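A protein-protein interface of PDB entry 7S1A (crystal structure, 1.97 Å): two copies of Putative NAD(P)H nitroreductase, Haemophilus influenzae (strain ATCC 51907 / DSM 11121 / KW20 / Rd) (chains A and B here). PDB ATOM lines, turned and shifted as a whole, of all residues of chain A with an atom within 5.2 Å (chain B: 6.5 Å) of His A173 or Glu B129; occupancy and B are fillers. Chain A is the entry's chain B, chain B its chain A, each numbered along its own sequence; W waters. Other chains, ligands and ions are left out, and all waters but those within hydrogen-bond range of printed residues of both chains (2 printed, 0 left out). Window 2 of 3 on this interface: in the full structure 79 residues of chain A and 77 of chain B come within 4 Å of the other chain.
Among the printed residues, merely in contact across the chains: His A173 with Asp B130 (3.4 Å), Phe A172 with Asp B130 (3.4 Å), Tyr A174 with Met B131 (3.7 Å) and His A173 with Lys B132 (3.9 Å).
No position is printed for both chains.
Of the 7 pairs that touch across the chains among the printed residues, none has its exchanged pair printed and touching as well.
NE2 of His A173 sits at hydrogen-bond distance from OE2 of Glu B129 (3.1 Å).
O of Asp B130 is in hydrogen-bond range of N of Tyr A174 (2.9 Å).
OD2 of Asp A175 is in salt-bridge range of NZ of Lys B132 (3.1 Å).
The backbone NH of Met B131 sits at hydrogen-bond distance from the backbone carbonyl oxygen of Leu B126.
The backbone carbonyl oxygen (O) of Gln B127 sits at hydrogen-bond distance from the backbone NH (N) of Lys B132 (3.2 Å).
NZ of Lys B132 is in salt-bridge range of OE2 of Glu B129 (3.2 Å).
N of His A173 lies within hydrogen-bond range of O of Phe A72 (3.0 Å).
A ring nitrogen (ND1) of His A173 lies within hydrogen-bond range of the backbone NH of Lys A176, 3.3 Å away.
O of Tyr A174 lies within hydrogen-bond range of ND2 of Asn A178 (3.1 Å).
Water W1 bridges OD1 of Asp B130 and O of Phe A72.
Water W2 lies within hydrogen-bond range of the side-chain amino group (NZ) of Lys B132 (2.8 Å), the backbone carbonyl oxygen (O) of Asp B130 (2.9 Å), the backbone NH (N) of Asp A175 (3.1 Å) and the backbone carbonyl oxygen (O) of Glu B129 (3.3 Å).
Of the printed residues of chain B, Phe A172 touches Asp B130 (3.4 Å).
Printed residues of chain B within 4 Å of His A173: Glu B129, Asp B130 and Lys B132.
Of the printed residues of chain B, Tyr A174 touches Asp B130 and Met B131.
Of the printed residues of chain B, Asp A175 touches Lys B132.
Of chain A, only His A173 (3.1 Å) comes within 4 Å of Glu B129.
Printed residues of chain A within 4 Å of Lys B132: His A173 (3.9 Å) and Asp A175 (3.1 Å).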
ATOM      1  N   PHE A  72      22.273  18.465 -15.648  1.00  0.00           N
ATOM      2  CA  PHE A  72      21.793  18.532 -14.272  1.00  0.00           C
ATOM      3  C   PHE A  72      22.866  18.184 -13.251  1.00  0.00           C
ATOM      4  O   PHE A  72      22.535  17.896 -12.101  1.00  0.00           O
ATOM      5  CB  PHE A  72      20.554  17.654 -14.052  1.00  0.00           C
ATOM      6  CG  PHE A  72      20.695  16.227 -14.502  1.00  0.00           C
ATOM      7  CD1 PHE A  72      21.246  15.267 -13.672  1.00  0.00           C
ATOM      8  CD2 PHE A  72      20.221  15.835 -15.746  1.00  0.00           C
ATOM      9  CE1 PHE A  72      21.354  13.946 -14.076  1.00  0.00           C
ATOM     10  CE2 PHE A  72      20.329  14.524 -16.151  1.00  0.00           C
ATOM     11  CZ  PHE A  72      20.891  13.578 -15.319  1.00  0.00           C
ATOM     12  N   SER A  73      24.147  18.235 -13.624  1.00  0.00           N
ATOM     13  CA  SER A  73      25.225  17.777 -12.748  1.00  0.00           C
ATOM     14  C   SER A  73      26.273  18.870 -12.627  1.00  0.00           C
ATOM     15  O   SER A  73      27.451  18.673 -12.928  1.00  0.00           O
ATOM     16  CB  SER A  73      25.847  16.485 -13.248  1.00  0.00           C
ATOM     17  OG  SER A  73      24.939  15.404 -13.133  1.00  0.00           O
ATOM     18  N   GLY A 171      26.921  17.425  -6.258  1.00  0.00           N
ATOM     19  CA  GLY A 171      26.407  18.523  -7.056  1.00  0.00           C
ATOM     20  C   GLY A 171      25.614  18.133  -8.281  1.00  0.00           C
ATOM     21  O   GLY A 171      26.046  18.399  -9.405  1.00  0.00           O
ATOM     22  N   PHE A 172      24.446  17.524  -8.077  1.00  0.00           N
ATOM     23  CA  PHE A 172      23.563  17.133  -9.174  1.00  0.00           C
ATOM     24  C   PHE A 172      22.140  17.016  -8.649  1.00  0.00           C
ATOM     25  O   PHE A 172      21.908  16.841  -7.449  1.00  0.00           O
ATOM     26  CB  PHE A 172      24.007  15.812  -9.836  1.00  0.00           C
ATOM     27  CG  PHE A 172      24.079  14.650  -8.891  1.00  0.00           C
ATOM     28  CD1 PHE A 172      22.950  13.896  -8.612  1.00  0.00           C
ATOM     29  CD2 PHE A 172      25.274  14.319  -8.270  1.00  0.00           C
ATOM     30  CE1 PHE A 172      23.015  12.821  -7.742  1.00  0.00           C
ATOM     31  CE2 PHE A 172      25.350  13.241  -7.405  1.00  0.00           C
ATOM     32  CZ  PHE A 172      24.210  12.497  -7.131  1.00  0.00           C
ATOM     33  N   HIS A 173      21.184  17.113  -9.572  1.00  0.00           N
ATOM     34  CA  HIS A 173      19.769  17.074  -9.221  1.00  0.00           C
ATOM     35  C   HIS A 173      19.393  15.617  -8.989  1.00  0.00           C
ATOM     36  O   HIS A 173      19.368  14.828  -9.932  1.00  0.00           O
ATOM     37  CB  HIS A 173      18.946  17.711 -10.343  1.00  0.00           C
ATOM     38  CG  HIS A 173      17.543  18.059  -9.954  1.00  0.00           C
ATOM     39  ND1 HIS A 173      16.522  17.133  -9.942  1.00  0.00           N
ATOM     40  CD2 HIS A 173      16.986  19.237  -9.574  1.00  0.00           C
ATOM     41  CE1 HIS A 173      15.398  17.722  -9.562  1.00  0.00           C
ATOM     42  NE2 HIS A 173      15.654  18.997  -9.328  1.00  0.00           N
ATOM     43  N   TYR A 174      19.113  15.246  -7.735  1.00  0.00           N
ATOM     44  CA  TYR A 174      18.970  13.831  -7.395  1.00  0.00           C
ATOM     45  C   TYR A 174      17.756  13.207  -8.082  1.00  0.00           C
ATOM     46  O   TYR A 174      17.842  12.095  -8.617  1.00  0.00           O
ATOM     47  CB  TYR A 174      18.908  13.673  -5.872  1.00  0.00           C
ATOM     48  CG  TYR A 174      20.266  13.484  -5.242  1.00  0.00           C
ATOM     49  CD1 TYR A 174      21.198  14.530  -5.216  1.00  0.00           C
ATOM     50  CD2 TYR A 174      20.641  12.257  -4.695  1.00  0.00           C
ATOM     51  CE1 TYR A 174      22.455  14.355  -4.665  1.00  0.00           C
ATOM     52  CE2 TYR A 174      21.881  12.084  -4.143  1.00  0.00           C
ATOM     53  CZ  TYR A 174      22.790  13.135  -4.136  1.00  0.00           C
ATOM     54  OH  TYR A 174      24.024  12.972  -3.577  1.00  0.00           O
ATOM     55  N   ASP A 175      16.632  13.931  -8.129  1.00  0.00           N
ATOM     56  CA  ASP A 175      15.444  13.422  -8.811  1.00  0.00           C
ATOM     57  C   ASP A 175      15.739  13.104 -10.270  1.00  0.00           C
ATOM     58  O   ASP A 175      15.342  12.047 -10.771  1.00  0.00           O
ATOM     59  CB  ASP A 175      14.282  14.424  -8.710  1.00  0.00           C
ATOM     60  CG  ASP A 175      13.569  14.366  -7.371  1.00  0.00           C
ATOM     61  OD1 ASP A 175      13.838  13.413  -6.599  1.00  0.00           O
ATOM     62  OD2 ASP A 175      12.738  15.265  -7.089  1.00  0.00           O
ATOM     63  N   LYS A 176      16.431  14.005 -10.973  1.00  0.00           N
ATOM     64  CA  LYS A 176      16.695  13.787 -12.396  1.00  0.00           C
ATOM     65  C   LYS A 176      17.726  12.684 -12.613  1.00  0.00           C
ATOM     66  O   LYS A 176      17.598  11.878 -13.542  1.00  0.00           O
ATOM     67  CB  LYS A 176      17.172  15.075 -13.062  1.00  0.00           C
ATOM     68  CG  LYS A 176      16.113  16.175 -13.221  1.00  0.00           C
ATOM     69  CD  LYS A 176      16.737  17.325 -13.998  1.00  0.00           C
ATOM     70  CE  LYS A 176      15.899  18.600 -14.014  1.00  0.00           C
ATOM     71  NZ  LYS A 176      16.732  19.737 -14.537  1.00  0.00           N
ATOM     72  N   MET A 177      18.756  12.640 -11.779  1.00  0.00           N
ATOM     73  CA  MET A 177      19.771  11.594 -11.875  1.00  0.00           C
ATOM     74  C   MET A 177      19.126  10.229 -11.657  1.00  0.00           C
ATOM     75  O   MET A 177      19.375   9.294 -12.422  1.00  0.00           O
ATOM     76  CB  MET A 177      20.893  11.839 -10.864  1.00  0.00           C
ATOM     77  CG  MET A 177      21.938  10.756 -10.831  1.00  0.00           C
ATOM     78  SD  MET A 177      23.160  10.919 -12.362  1.00  0.00           S
ATOM     79  CE  MET A 177      24.180  12.522 -11.778  1.00  0.00           C
ATOM     80  N   ASN A 178      18.287  10.122 -10.620  1.00  0.00           N
ATOM     81  CA  ASN A 178      17.543   8.885 -10.391  1.00  0.00           C
ATOM     82  C   ASN A 178      16.745   8.498 -11.626  1.00  0.00           C
ATOM     83  O   ASN A 178      16.803   7.356 -12.092  1.00  0.00           O
ATOM     84  CB  ASN A 178      16.614   9.036  -9.189  1.00  0.00           C
ATOM     85  CG  ASN A 178      17.293   8.665  -7.872  1.00  0.00           C
ATOM     86  OD1 ASN A 178      17.867   7.579  -7.743  1.00  0.00           O
ATOM     87  ND2 ASN A 178      17.227   9.566  -6.887  1.00  0.00           N
ATOM     88  N   LYS B 124      21.922  27.183  -1.711  1.00  0.00           N
ATOM     89  CA  LYS B 124      20.463  27.189  -1.661  1.00  0.00           C
ATOM     90  C   LYS B 124      19.896  26.220  -2.682  1.00  0.00           C
ATOM     91  O   LYS B 124      19.065  25.370  -2.348  1.00  0.00           O
ATOM     92  CB  LYS B 124      19.948  28.603  -1.898  1.00  0.00           C
ATOM     93  CG  LYS B 124      18.433  28.727  -2.080  1.00  0.00           C
ATOM     94  CD  LYS B 124      18.058  30.178  -2.331  1.00  0.00           C
ATOM     95  CE  LYS B 124      16.654  30.312  -2.890  1.00  0.00           C
ATOM     96  NZ  LYS B 124      15.656  30.166  -1.814  1.00  0.00           N
ATOM     97  N   ALA B 125      20.366  26.317  -3.929  1.00  0.00           N
ATOM     98  CA  ALA B 125      19.996  25.365  -4.968  1.00  0.00           C
ATOM     99  C   ALA B 125      20.264  23.935  -4.526  1.00  0.00           C
ATOM    100  O   ALA B 125      19.377  23.077  -4.598  1.00  0.00           O
ATOM    101  CB  ALA B 125      20.778  25.655  -6.248  1.00  0.00           C
ATOM    102  N   LEU B 126      21.503  23.650  -4.116  1.00  0.00           N
ATOM    103  CA  LEU B 126      21.846  22.307  -3.646  1.00  0.00           C
ATOM    104  C   LEU B 126      20.870  21.824  -2.580  1.00  0.00           C
ATOM    105  O   LEU B 126      20.309  20.724  -2.680  1.00  0.00           O
ATOM    106  CB  LEU B 126      23.279  22.275  -3.101  1.00  0.00           C
ATOM    107  CG  LEU B 126      23.702  20.885  -2.614  1.00  0.00           C
ATOM    108  CD1 LEU B 126      23.871  19.900  -3.795  1.00  0.00           C
ATOM    109  CD2 LEU B 126      24.959  20.926  -1.784  1.00  0.00           C
ATOM    110  N   GLN B 127      20.658  22.630  -1.544  1.00  0.00           N
ATOM    111  CA  GLN B 127      19.852  22.164  -0.416  1.00  0.00           C
ATOM    112  C   GLN B 127      18.368  22.142  -0.748  1.00  0.00           C
ATOM    113  O   GLN B 127      17.678  21.154  -0.480  1.00  0.00           O
ATOM    114  CB  GLN B 127      20.082  23.053   0.798  1.00  0.00           C
ATOM    115  CG  GLN B 127      21.465  22.920   1.338  1.00  0.00           C
ATOM    116  CD  GLN B 127      21.602  23.638   2.669  1.00  0.00           C
ATOM    117  OE1 GLN B 127      20.906  24.617   2.928  1.00  0.00           O
ATOM    118  NE2 GLN B 127      22.493  23.139   3.527  1.00  0.00           N
ATOM    119  N   GLU B 128      17.866  23.225  -1.327  1.00  0.00           N
ATOM    120  CA  GLU B 128      16.431  23.361  -1.546  1.00  0.00           C
ATOM    121  C   GLU B 128      15.949  22.468  -2.683  1.00  0.00           C
ATOM    122  O   GLU B 128      14.883  21.856  -2.580  1.00  0.00           O
ATOM    123  CB  GLU B 128      16.078  24.825  -1.844  1.00  0.00           C
ATOM    124  CG  GLU B 128      14.718  25.242  -1.357  1.00  0.00           C
ATOM    125  CD  GLU B 128      14.444  26.723  -1.524  1.00  0.00           C
ATOM    126  OE1 GLU B 128      15.058  27.358  -2.417  1.00  0.00           O
ATOM    127  OE2 GLU B 128      13.603  27.245  -0.756  1.00  0.00           O
ATOM    128  N   GLU B 129      16.698  22.398  -3.785  1.00  0.00           N
ATOM    129  CA  GLU B 129      16.161  21.803  -5.006  1.00  0.00           C
ATOM    130  C   GLU B 129      16.871  20.527  -5.426  1.00  0.00           C
ATOM    131  O   GLU B 129      16.200  19.535  -5.740  1.00  0.00           O
ATOM    132  CB  GLU B 129      16.193  22.807  -6.176  1.00  0.00           C
ATOM    133  CG  GLU B 129      15.586  22.258  -7.482  1.00  0.00           C
ATOM    134  CD  GLU B 129      14.087  21.919  -7.366  1.00  0.00           C
ATOM    135  OE1 GLU B 129      13.286  22.802  -6.958  1.00  0.00           O
ATOM    136  OE2 GLU B 129      13.703  20.769  -7.703  1.00  0.00           O
ATOM    137  N   ASP B 130      18.204  20.521  -5.476  1.00  0.00           N
ATOM    138  CA  ASP B 130      18.904  19.354  -6.002  1.00  0.00           C
ATOM    139  C   ASP B 130      18.812  18.179  -5.040  1.00  0.00           C
ATOM    140  O   ASP B 130      18.596  17.031  -5.465  1.00  0.00           O
ATOM    141  CB  ASP B 130      20.373  19.667  -6.261  1.00  0.00           C
ATOM    142  CG  ASP B 130      20.579  20.629  -7.393  1.00  0.00           C
ATOM    143  OD1 ASP B 130      19.793  20.622  -8.368  1.00  0.00           O
ATOM    144  OD2 ASP B 130      21.548  21.406  -7.297  1.00  0.00           O
ATOM    145  N   MET B 131      19.012  18.437  -3.749  1.00  0.00           N
ATOM    146  CA  MET B 131      18.995  17.369  -2.764  1.00  0.00           C
ATOM    147  C   MET B 131      17.749  17.406  -1.869  1.00  0.00           C
ATOM    148  O   MET B 131      17.532  16.481  -1.108  1.00  0.00           O
ATOM    149  CB  MET B 131      20.263  17.417  -1.895  1.00  0.00           C
ATOM    150  CG  MET B 131      21.620  17.362  -2.658  1.00  0.00           C
ATOM    151  SD  MET B 131      23.109  17.137  -1.470  1.00  0.00           S
ATOM    152  CE  MET B 131      22.839  15.318  -0.868  1.00  0.00           C
ATOM    153  N   LYS B 132      16.939  18.459  -1.950  1.00  0.00           N
ATOM    154  CA  LYS B 132      15.662  18.523  -1.228  1.00  0.00           C
ATOM    155  C   LYS B 132      15.837  18.228   0.265  1.00  0.00           C
ATOM    156  O   LYS B 132      15.161  17.373   0.855  1.00  0.00           O
ATOM    157  CB  LYS B 132      14.641  17.584  -1.872  1.00  0.00           C
ATOM    158  CG  LYS B 132      14.306  17.992  -3.314  1.00  0.00           C
ATOM    159  CD  LYS B 132      13.187  17.161  -3.888  1.00  0.00           C
ATOM    160  CE  LYS B 132      12.639  17.864  -5.105  1.00  0.00           C
ATOM    161  NZ  LYS B 132      13.736  18.028  -6.073  1.00  0.00           N
ATOM    162  N   LEU B 133      16.770  18.953   0.878  1.00  0.00           N
ATOM    163  CA  LEU B 133      17.139  18.743   2.274  1.00  0.00           C
ATOM    164  C   LEU B 133      16.339  19.595   3.243  1.00  0.00           C
ATOM    165  O   LEU B 133      16.449  19.388   4.460  1.00  0.00           O
ATOM    166  CB  LEU B 133      18.617  19.063   2.493  1.00  0.00           C
ATOM    167  CG  LEU B 133      19.654  18.389   1.625  1.00  0.00           C
ATOM    168  CD1 LEU B 133      21.011  18.917   2.026  1.00  0.00           C
ATOM    169  CD2 LEU B 133      19.580  16.867   1.802  1.00  0.00           C
HETATM  170  O   HOH W   1      21.035  20.768 -10.897  1.00  0.00           O
HETATM  171  O   HOH W   2      15.937  16.230  -6.119  1.00  0.00           O
